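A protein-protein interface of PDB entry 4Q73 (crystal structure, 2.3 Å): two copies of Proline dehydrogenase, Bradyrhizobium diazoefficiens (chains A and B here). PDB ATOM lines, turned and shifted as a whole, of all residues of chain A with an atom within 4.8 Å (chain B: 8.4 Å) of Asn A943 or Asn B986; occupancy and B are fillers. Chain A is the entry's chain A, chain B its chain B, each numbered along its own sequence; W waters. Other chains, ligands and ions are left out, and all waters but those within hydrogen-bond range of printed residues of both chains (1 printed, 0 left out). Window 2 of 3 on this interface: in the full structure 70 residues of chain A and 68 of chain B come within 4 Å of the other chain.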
ATOM      1  N   LYS A 353     -33.892   6.729  -5.244  1.00  0.00           N
ATOM      2  CA  LYS A 353     -33.469   7.874  -4.454  1.00  0.00           C
ATOM      3  C   LYS A 353     -33.408   9.115  -5.315  1.00  0.00           C
ATOM      4  O   LYS A 353     -33.980  10.178  -4.968  1.00  0.00           O
ATOM      5  CB  LYS A 353     -32.093   7.587  -3.822  1.00  0.00           C
ATOM      6  CG  LYS A 353     -31.601   8.689  -2.887  1.00  0.00           C
ATOM      7  CD  LYS A 353     -30.470   8.243  -1.978  1.00  0.00           C
ATOM      8  CE  LYS A 353     -30.029   9.407  -1.100  1.00  0.00           C
ATOM      9  NZ  LYS A 353     -29.058   9.024  -0.036  1.00  0.00           N
ATOM     10  N   ASP A 781     -18.275  15.206  -3.327  1.00  0.00           N
ATOM     11  CA  ASP A 781     -19.053  15.990  -2.377  1.00  0.00           C
ATOM     12  C   ASP A 781     -18.342  17.269  -1.934  1.00  0.00           C
ATOM     13  O   ASP A 781     -18.994  18.243  -1.571  1.00  0.00           O
ATOM     14  CB  ASP A 781     -19.432  15.138  -1.159  1.00  0.00           C
ATOM     15  CG  ASP A 781     -20.449  14.045  -1.493  1.00  0.00           C
ATOM     16  OD1 ASP A 781     -21.163  14.180  -2.513  1.00  0.00           O
ATOM     17  OD2 ASP A 781     -20.526  13.050  -0.731  1.00  0.00           O
ATOM     18  N   VAL A 920     -19.441  15.274   7.550  1.00  0.00           N
ATOM     19  CA  VAL A 920     -18.599  14.209   8.079  1.00  0.00           C
ATOM     20  C   VAL A 920     -18.619  13.033   7.112  1.00  0.00           C
ATOM     21  O   VAL A 920     -19.687  12.545   6.720  1.00  0.00           O
ATOM     22  CB  VAL A 920     -19.036  13.730   9.480  1.00  0.00           C
ATOM     23  CG1 VAL A 920     -18.033  12.695  10.006  1.00  0.00           C
ATOM     24  CG2 VAL A 920     -19.125  14.897  10.444  1.00  0.00           C
ATOM     25  N   HIS A 921     -17.426  12.604   6.715  1.00  0.00           N
ATOM     26  CA  HIS A 921     -17.245  11.472   5.813  1.00  0.00           C
ATOM     27  C   HIS A 921     -16.431  10.396   6.500  1.00  0.00           C
ATOM     28  O   HIS A 921     -15.223  10.559   6.736  1.00  0.00           O
ATOM     29  CB  HIS A 921     -16.548  11.895   4.528  1.00  0.00           C
ATOM     30  CG  HIS A 921     -17.467  12.023   3.361  1.00  0.00           C
ATOM     31  ND1 HIS A 921     -18.173  13.171   3.085  1.00  0.00           N
ATOM     32  CD2 HIS A 921     -17.803  11.134   2.386  1.00  0.00           C
ATOM     33  CE1 HIS A 921     -18.899  12.995   1.992  1.00  0.00           C
ATOM     34  NE2 HIS A 921     -18.682  11.761   1.554  1.00  0.00           N
ATOM     35  N   SER A 922     -17.104   9.295   6.807  1.00  0.00           N
ATOM     36  CA  SER A 922     -16.501   8.225   7.565  1.00  0.00           C
ATOM     37  C   SER A 922     -17.371   6.994   7.499  1.00  0.00           C
ATOM     38  O   SER A 922     -18.580   7.107   7.334  1.00  0.00           O
ATOM     39  CB  SER A 922     -16.333   8.660   9.014  1.00  0.00           C
ATOM     40  OG  SER A 922     -15.978   7.572   9.835  1.00  0.00           O
ATOM     41  N   ILE A 928     -18.633   9.142  13.902  1.00  0.00           N
ATOM     42  CA  ILE A 928     -19.678  10.069  13.475  1.00  0.00           C
ATOM     43  C   ILE A 928     -20.494  10.550  14.658  1.00  0.00           C
ATOM     44  O   ILE A 928     -20.748  11.755  14.825  1.00  0.00           O
ATOM     45  CB  ILE A 928     -20.622   9.395  12.471  1.00  0.00           C
ATOM     46  CG1 ILE A 928     -19.870   9.114  11.171  1.00  0.00           C
ATOM     47  CG2 ILE A 928     -21.859  10.268  12.202  1.00  0.00           C
ATOM     48  CD1 ILE A 928     -20.595   8.164  10.263  1.00  0.00           C
ATOM     49  N   TYR A 941     -24.176  16.923   7.983  1.00  0.00           N
ATOM     50  CA  TYR A 941     -24.376  16.064   6.820  1.00  0.00           C
ATOM     51  C   TYR A 941     -23.322  14.979   6.788  1.00  0.00           C
ATOM     52  O   TYR A 941     -22.124  15.254   6.819  1.00  0.00           O
ATOM     53  CB  TYR A 941     -24.298  16.864   5.522  1.00  0.00           C
ATOM     54  CG  TYR A 941     -25.432  17.828   5.289  1.00  0.00           C
ATOM     55  CD1 TYR A 941     -25.319  19.168   5.650  1.00  0.00           C
ATOM     56  CD2 TYR A 941     -26.594  17.414   4.656  1.00  0.00           C
ATOM     57  CE1 TYR A 941     -26.341  20.064   5.409  1.00  0.00           C
ATOM     58  CE2 TYR A 941     -27.633  18.293   4.420  1.00  0.00           C
ATOM     59  CZ  TYR A 941     -27.501  19.622   4.791  1.00  0.00           C
ATOM     60  OH  TYR A 941     -28.530  20.515   4.549  1.00  0.00           O
ATOM     61  N   VAL A 942     -23.784  13.742   6.715  1.00  0.00           N
ATOM     62  CA  VAL A 942     -22.904  12.607   6.838  1.00  0.00           C
ATOM     63  C   VAL A 942     -22.875  11.802   5.552  1.00  0.00           C
ATOM     64  O   VAL A 942     -23.914  11.379   5.057  1.00  0.00           O
ATOM     65  CB  VAL A 942     -23.332  11.716   7.996  1.00  0.00           C
ATOM     66  CG1 VAL A 942     -22.321  10.580   8.184  1.00  0.00           C
ATOM     67  CG2 VAL A 942     -23.428  12.557   9.230  1.00  0.00           C
ATOM     68  N   ASN A 943     -21.678  11.627   5.016  1.00  0.00           N
ATOM     69  CA  ASN A 943     -21.470  10.900   3.773  1.00  0.00           C
ATOM     70  C   ASN A 943     -22.274  11.417   2.574  1.00  0.00           C
ATOM     71  O   ASN A 943     -22.708  10.653   1.716  1.00  0.00           O
ATOM     72  CB  ASN A 943     -21.627   9.393   4.006  1.00  0.00           C
ATOM     73  CG  ASN A 943     -20.571   8.861   4.973  1.00  0.00           C
ATOM     74  OD1 ASN A 943     -19.428   9.363   5.007  1.00  0.00           O
ATOM     75  ND2 ASN A 943     -20.941   7.868   5.775  1.00  0.00           N
ATOM     76  N   ARG A 944     -22.466  12.729   2.532  1.00  0.00           N
ATOM     77  CA  ARG A 944     -23.012  13.404   1.352  1.00  0.00           C
ATOM     78  C   ARG A 944     -22.554  14.873   1.337  1.00  0.00           C
ATOM     79  O   ARG A 944     -21.835  15.311   2.238  1.00  0.00           O
ATOM     80  CB  ARG A 944     -24.539  13.304   1.339  1.00  0.00           C
ATOM     81  CG  ARG A 944     -25.220  13.708   2.652  1.00  0.00           C
ATOM     82  CD  ARG A 944     -26.649  14.218   2.387  1.00  0.00           C
ATOM     83  NE  ARG A 944     -26.609  15.569   1.815  1.00  0.00           N
ATOM     84  CZ  ARG A 944     -27.670  16.265   1.418  1.00  0.00           C
ATOM     85  NH1 ARG A 944     -27.495  17.484   0.919  1.00  0.00           N
ATOM     86  NH2 ARG A 944     -28.896  15.749   1.520  1.00  0.00           N
ATOM     87  N   THR B 639     -35.814   7.980   0.174  1.00  0.00           N
ATOM     88  CA  THR B 639     -35.259   6.699   0.578  1.00  0.00           C
ATOM     89  C   THR B 639     -33.714   6.805   0.557  1.00  0.00           C
ATOM     90  O   THR B 639     -33.163   7.728  -0.065  1.00  0.00           O
ATOM     91  CB  THR B 639     -35.720   5.599  -0.385  1.00  0.00           C
ATOM     92  OG1 THR B 639     -35.347   4.322   0.133  1.00  0.00           O
ATOM     93  CG2 THR B 639     -35.072   5.793  -1.746  1.00  0.00           C
ATOM     94  N   GLY B 640     -33.018   5.900   1.251  1.00  0.00           N
ATOM     95  CA  GLY B 640     -31.559   5.935   1.300  1.00  0.00           C
ATOM     96  C   GLY B 640     -30.952   7.108   2.082  1.00  0.00           C
ATOM     97  O   GLY B 640     -29.760   7.389   1.957  1.00  0.00           O
ATOM     98  N   GLU B 641     -31.764   7.802   2.886  1.00  0.00           N
ATOM     99  CA  GLU B 641     -31.305   8.956   3.668  1.00  0.00           C
ATOM    100  C   GLU B 641     -32.140   9.136   4.930  1.00  0.00           C
ATOM    101  O   GLU B 641     -33.361   9.116   4.863  1.00  0.00           O
ATOM    102  CB  GLU B 641     -31.391  10.249   2.841  1.00  0.00           C
ATOM    103  CG  GLU B 641     -30.653  11.439   3.468  1.00  0.00           C
ATOM    104  CD  GLU B 641     -30.876  12.771   2.717  1.00  0.00           C
ATOM    105  OE1 GLU B 641     -31.987  13.368   2.837  1.00  0.00           O
ATOM    106  OE2 GLU B 641     -29.947  13.215   1.997  1.00  0.00           O
ATOM    107  N   SER B 642     -31.496   9.356   6.072  1.00  0.00           N
ATOM    108  CA  SER B 642     -32.243   9.675   7.283  1.00  0.00           C
ATOM    109  C   SER B 642     -32.042  11.146   7.686  1.00  0.00           C
ATOM    110  O   SER B 642     -30.953  11.715   7.530  1.00  0.00           O
ATOM    111  CB  SER B 642     -31.861   8.741   8.432  1.00  0.00           C
ATOM    112  OG  SER B 642     -30.597   9.074   8.973  1.00  0.00           O
ATOM    113  N   ASN B 643     -33.111  11.746   8.202  1.00  0.00           N
ATOM    114  CA  ASN B 643     -33.116  13.126   8.657  1.00  0.00           C
ATOM    115  C   ASN B 643     -33.801  13.214  10.017  1.00  0.00           C
ATOM    116  O   ASN B 643     -34.968  12.841  10.141  1.00  0.00           O
ATOM    117  CB  ASN B 643     -33.833  14.025   7.652  1.00  0.00           C
ATOM    118  CG  ASN B 643     -33.105  14.121   6.320  1.00  0.00           C
ATOM    119  OD1 ASN B 643     -32.220  14.959   6.129  1.00  0.00           O
ATOM    120  ND2 ASN B 643     -33.482  13.261   5.391  1.00  0.00           N
ATOM    121  N   VAL B 983     -29.523  16.305  11.740  1.00  0.00           N
ATOM    122  CA  VAL B 983     -28.490  15.372  11.330  1.00  0.00           C
ATOM    123  C   VAL B 983     -28.991  14.629  10.114  1.00  0.00           C
ATOM    124  O   VAL B 983     -30.055  14.010  10.156  1.00  0.00           O
ATOM    125  CB  VAL B 983     -28.134  14.378  12.448  1.00  0.00           C
ATOM    126  CG1 VAL B 983     -27.345  13.203  11.880  1.00  0.00           C
ATOM    127  CG2 VAL B 983     -27.379  15.096  13.595  1.00  0.00           C
ATOM    128  N   THR B 984     -28.246  14.735   9.020  1.00  0.00           N
ATOM    129  CA  THR B 984     -28.646  14.157   7.748  1.00  0.00           C
ATOM    130  C   THR B 984     -27.614  13.145   7.311  1.00  0.00           C
ATOM    131  O   THR B 984     -26.477  13.482   7.013  1.00  0.00           O
ATOM    132  CB  THR B 984     -28.822  15.231   6.649  1.00  0.00           C
ATOM    133  OG1 THR B 984     -29.893  16.118   7.010  1.00  0.00           O
ATOM    134  CG2 THR B 984     -29.119  14.596   5.285  1.00  0.00           C
ATOM    135  N   ILE B 985     -28.028  11.891   7.285  1.00  0.00           N
ATOM    136  CA  ILE B 985     -27.133  10.805   6.978  1.00  0.00           C
ATOM    137  C   ILE B 985     -27.556  10.081   5.711  1.00  0.00           C
ATOM    138  O   ILE B 985     -28.693   9.650   5.583  1.00  0.00           O
ATOM    139  CB  ILE B 985     -27.095   9.792   8.107  1.00  0.00           C
ATOM    140  CG1 ILE B 985     -26.769  10.479   9.427  1.00  0.00           C
ATOM    141  CG2 ILE B 985     -26.094   8.644   7.777  1.00  0.00           C
ATOM    142  CD1 ILE B 985     -26.738   9.540  10.604  1.00  0.00           C
ATOM    143  N   ASN B 986     -26.621   9.976   4.776  1.00  0.00           N
ATOM    144  CA  ASN B 986     -26.780   9.184   3.577  1.00  0.00           C
ATOM    145  C   ASN B 986     -26.579   7.717   3.928  1.00  0.00           C
ATOM    146  O   ASN B 986     -25.462   7.271   4.187  1.00  0.00           O
ATOM    147  CB  ASN B 986     -25.792   9.683   2.522  1.00  0.00           C
ATOM    148  CG  ASN B 986     -25.682   8.778   1.320  1.00  0.00           C
ATOM    149  OD1 ASN B 986     -26.430   7.804   1.151  1.00  0.00           O
ATOM    150  ND2 ASN B 986     -24.711   9.093   0.466  1.00  0.00           N
ATOM    151  N   THR B 987     -27.676   6.973   3.921  1.00  0.00           N
ATOM    152  CA  THR B 987     -27.683   5.623   4.451  1.00  0.00           C
ATOM    153  C   THR B 987     -27.634   4.596   3.338  1.00  0.00           C
ATOM    154  O   THR B 987     -27.770   3.404   3.607  1.00  0.00           O
ATOM    155  CB  THR B 987     -28.958   5.358   5.342  1.00  0.00           C
ATOM    156  OG1 THR B 987     -30.150   5.648   4.602  1.00  0.00           O
ATOM    157  CG2 THR B 987     -28.959   6.233   6.600  1.00  0.00           C
ATOM    158  N   ALA B 988     -27.439   5.036   2.091  1.00  0.00           N
ATOM    159  CA  ALA B 988     -27.582   4.112   0.951  1.00  0.00           C
ATOM    160  C   ALA B 988     -26.615   2.933   0.939  1.00  0.00           C
ATOM    161  O   ALA B 988     -26.972   1.850   0.452  1.00  0.00           O
ATOM    162  CB  ALA B 988     -27.519   4.840  -0.384  1.00  0.00           C
ATOM    163  N   ALA B 989     -25.401   3.112   1.456  1.00  0.00           N
ATOM    164  CA  ALA B 989     -24.441   1.997   1.439  1.00  0.00           C
ATOM    165  C   ALA B 989     -24.851   0.867   2.389  1.00  0.00           C
ATOM    166  O   ALA B 989     -24.246  -0.206   2.373  1.00  0.00           O
ATOM    167  CB  ALA B 989     -23.029   2.475   1.745  1.00  0.00           C
ATOM    168  N   ALA B 990     -25.877   1.110   3.208  1.00  0.00           N
ATOM    169  CA  ALA B 990     -26.380   0.096   4.133  1.00  0.00           C
ATOM    170  C   ALA B 990     -27.648  -0.562   3.595  1.00  0.00           C
ATOM    171  O   ALA B 990     -27.984  -1.684   3.976  1.00  0.00           O
ATOM    172  CB  ALA B 990     -26.653   0.721   5.494  1.00  0.00           C
ATOM    173  N   GLY B 991     -28.325   0.127   2.679  1.00  0.00           N
ATOM    174  CA  GLY B 991     -29.669  -0.237   2.269  1.00  0.00           C
ATOM    175  C   GLY B 991     -30.714   0.655   2.914  1.00  0.00           C
ATOM    176  O   GLY B 991     -30.386   1.648   3.575  1.00  0.00           O
HETATM  177  O   HOH W   1     -28.089  11.371   1.135  1.00  0.00           O
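The backbone NH of Val A942 sits at hydrogen-bond distance from the backbone carbonyl oxygen of Thr B984, at 2.7 Å. O of Gly B640 sits at hydrogen-bond distance from NZ of Lys A353 (2.7 Å). O of Asn A943 is in hydrogen-bond range of ND2 of Asn B986 (2.8 Å). N of Asn B986 sits at hydrogen-bond distance from O of Val A942 (3.1 Å). The side-chain amino group (NZ) of Lys A353 sits at hydrogen-bond distance from the side-chain amide oxygen (OD1) of Asn B986 (3.1 Å). The guanidinium group (NH2) of Arg A944 is in salt-bridge range of the side-chain carboxylate (OE2) of Glu B641 (2.8 Å).
Of the 10 printed residues of chain A, 5 touch a printed residue of chain B. Of the 14 printed residues of chain B, 6 touch a printed residue of chain A.
The backbone NH (N) of Val A920 lies within hydrogen-bond range of the backbone carbonyl oxygen (O) of Tyr A941. N of Thr B987 is in hydrogen-bond range of O of Gly B640. The backbone NH (N) of Asn A943 is in hydrogen-bond range of the backbone carbonyl oxygen (O) of Val A920 (2.8 Å). The backbone carbonyl oxygen of Ser A922 sits at hydrogen-bond distance from the side-chain amide nitrogen of Asn A943 (2.9 Å). The backbone NH (N) of Glu B641 lies within hydrogen-bond range of the side-chain hydroxyl (OG1) of Thr B987. The backbone carbonyl oxygen (O) of Gly B640 lies close to the side-chain amide oxygen (OD1) of Asn B986 (3.5 Å).
Water W1 bridges OE2 of Glu B641 (2.8 Å) and NZ of Lys A353 (2.8 Å).
No position is printed for both chains.
Asn A943 touches one residue of chain B. Of the printed residues of chain A, Asn B986 touches Lys A353 (3.1 Å), Val A942 (3.1 Å) and Asn A943 (2.8 Å). Of the printed residues of chain B, Val A942 touches Thr B984 (2.7 Å), Ile B985 (3.8 Å) and Asn B986 (3.1 Å). Of the printed residues of chain B, Tyr A941 touches Thr B984. Of the printed residues of chain A, Thr B639 touches Lys A353 (3.3 Å). Printed residues of chain A within 4 Å of Thr B984: Tyr A941, Val A942 and Arg A944. The nearest printed residue of chain B that does not touch Lys A353 is Ala B988 (4.5 Å).
Among the printed residues, merely in contact across the chains: Lys A353 with Thr B639 (3.3 Å), Lys A353 with Glu B641 (3.9 Å), Tyr A941 with Thr B984 (3.3 Å), Val A942 with Ile B985 (3.8 Å) and Arg A944 with Thr B984 (3.8 Å).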
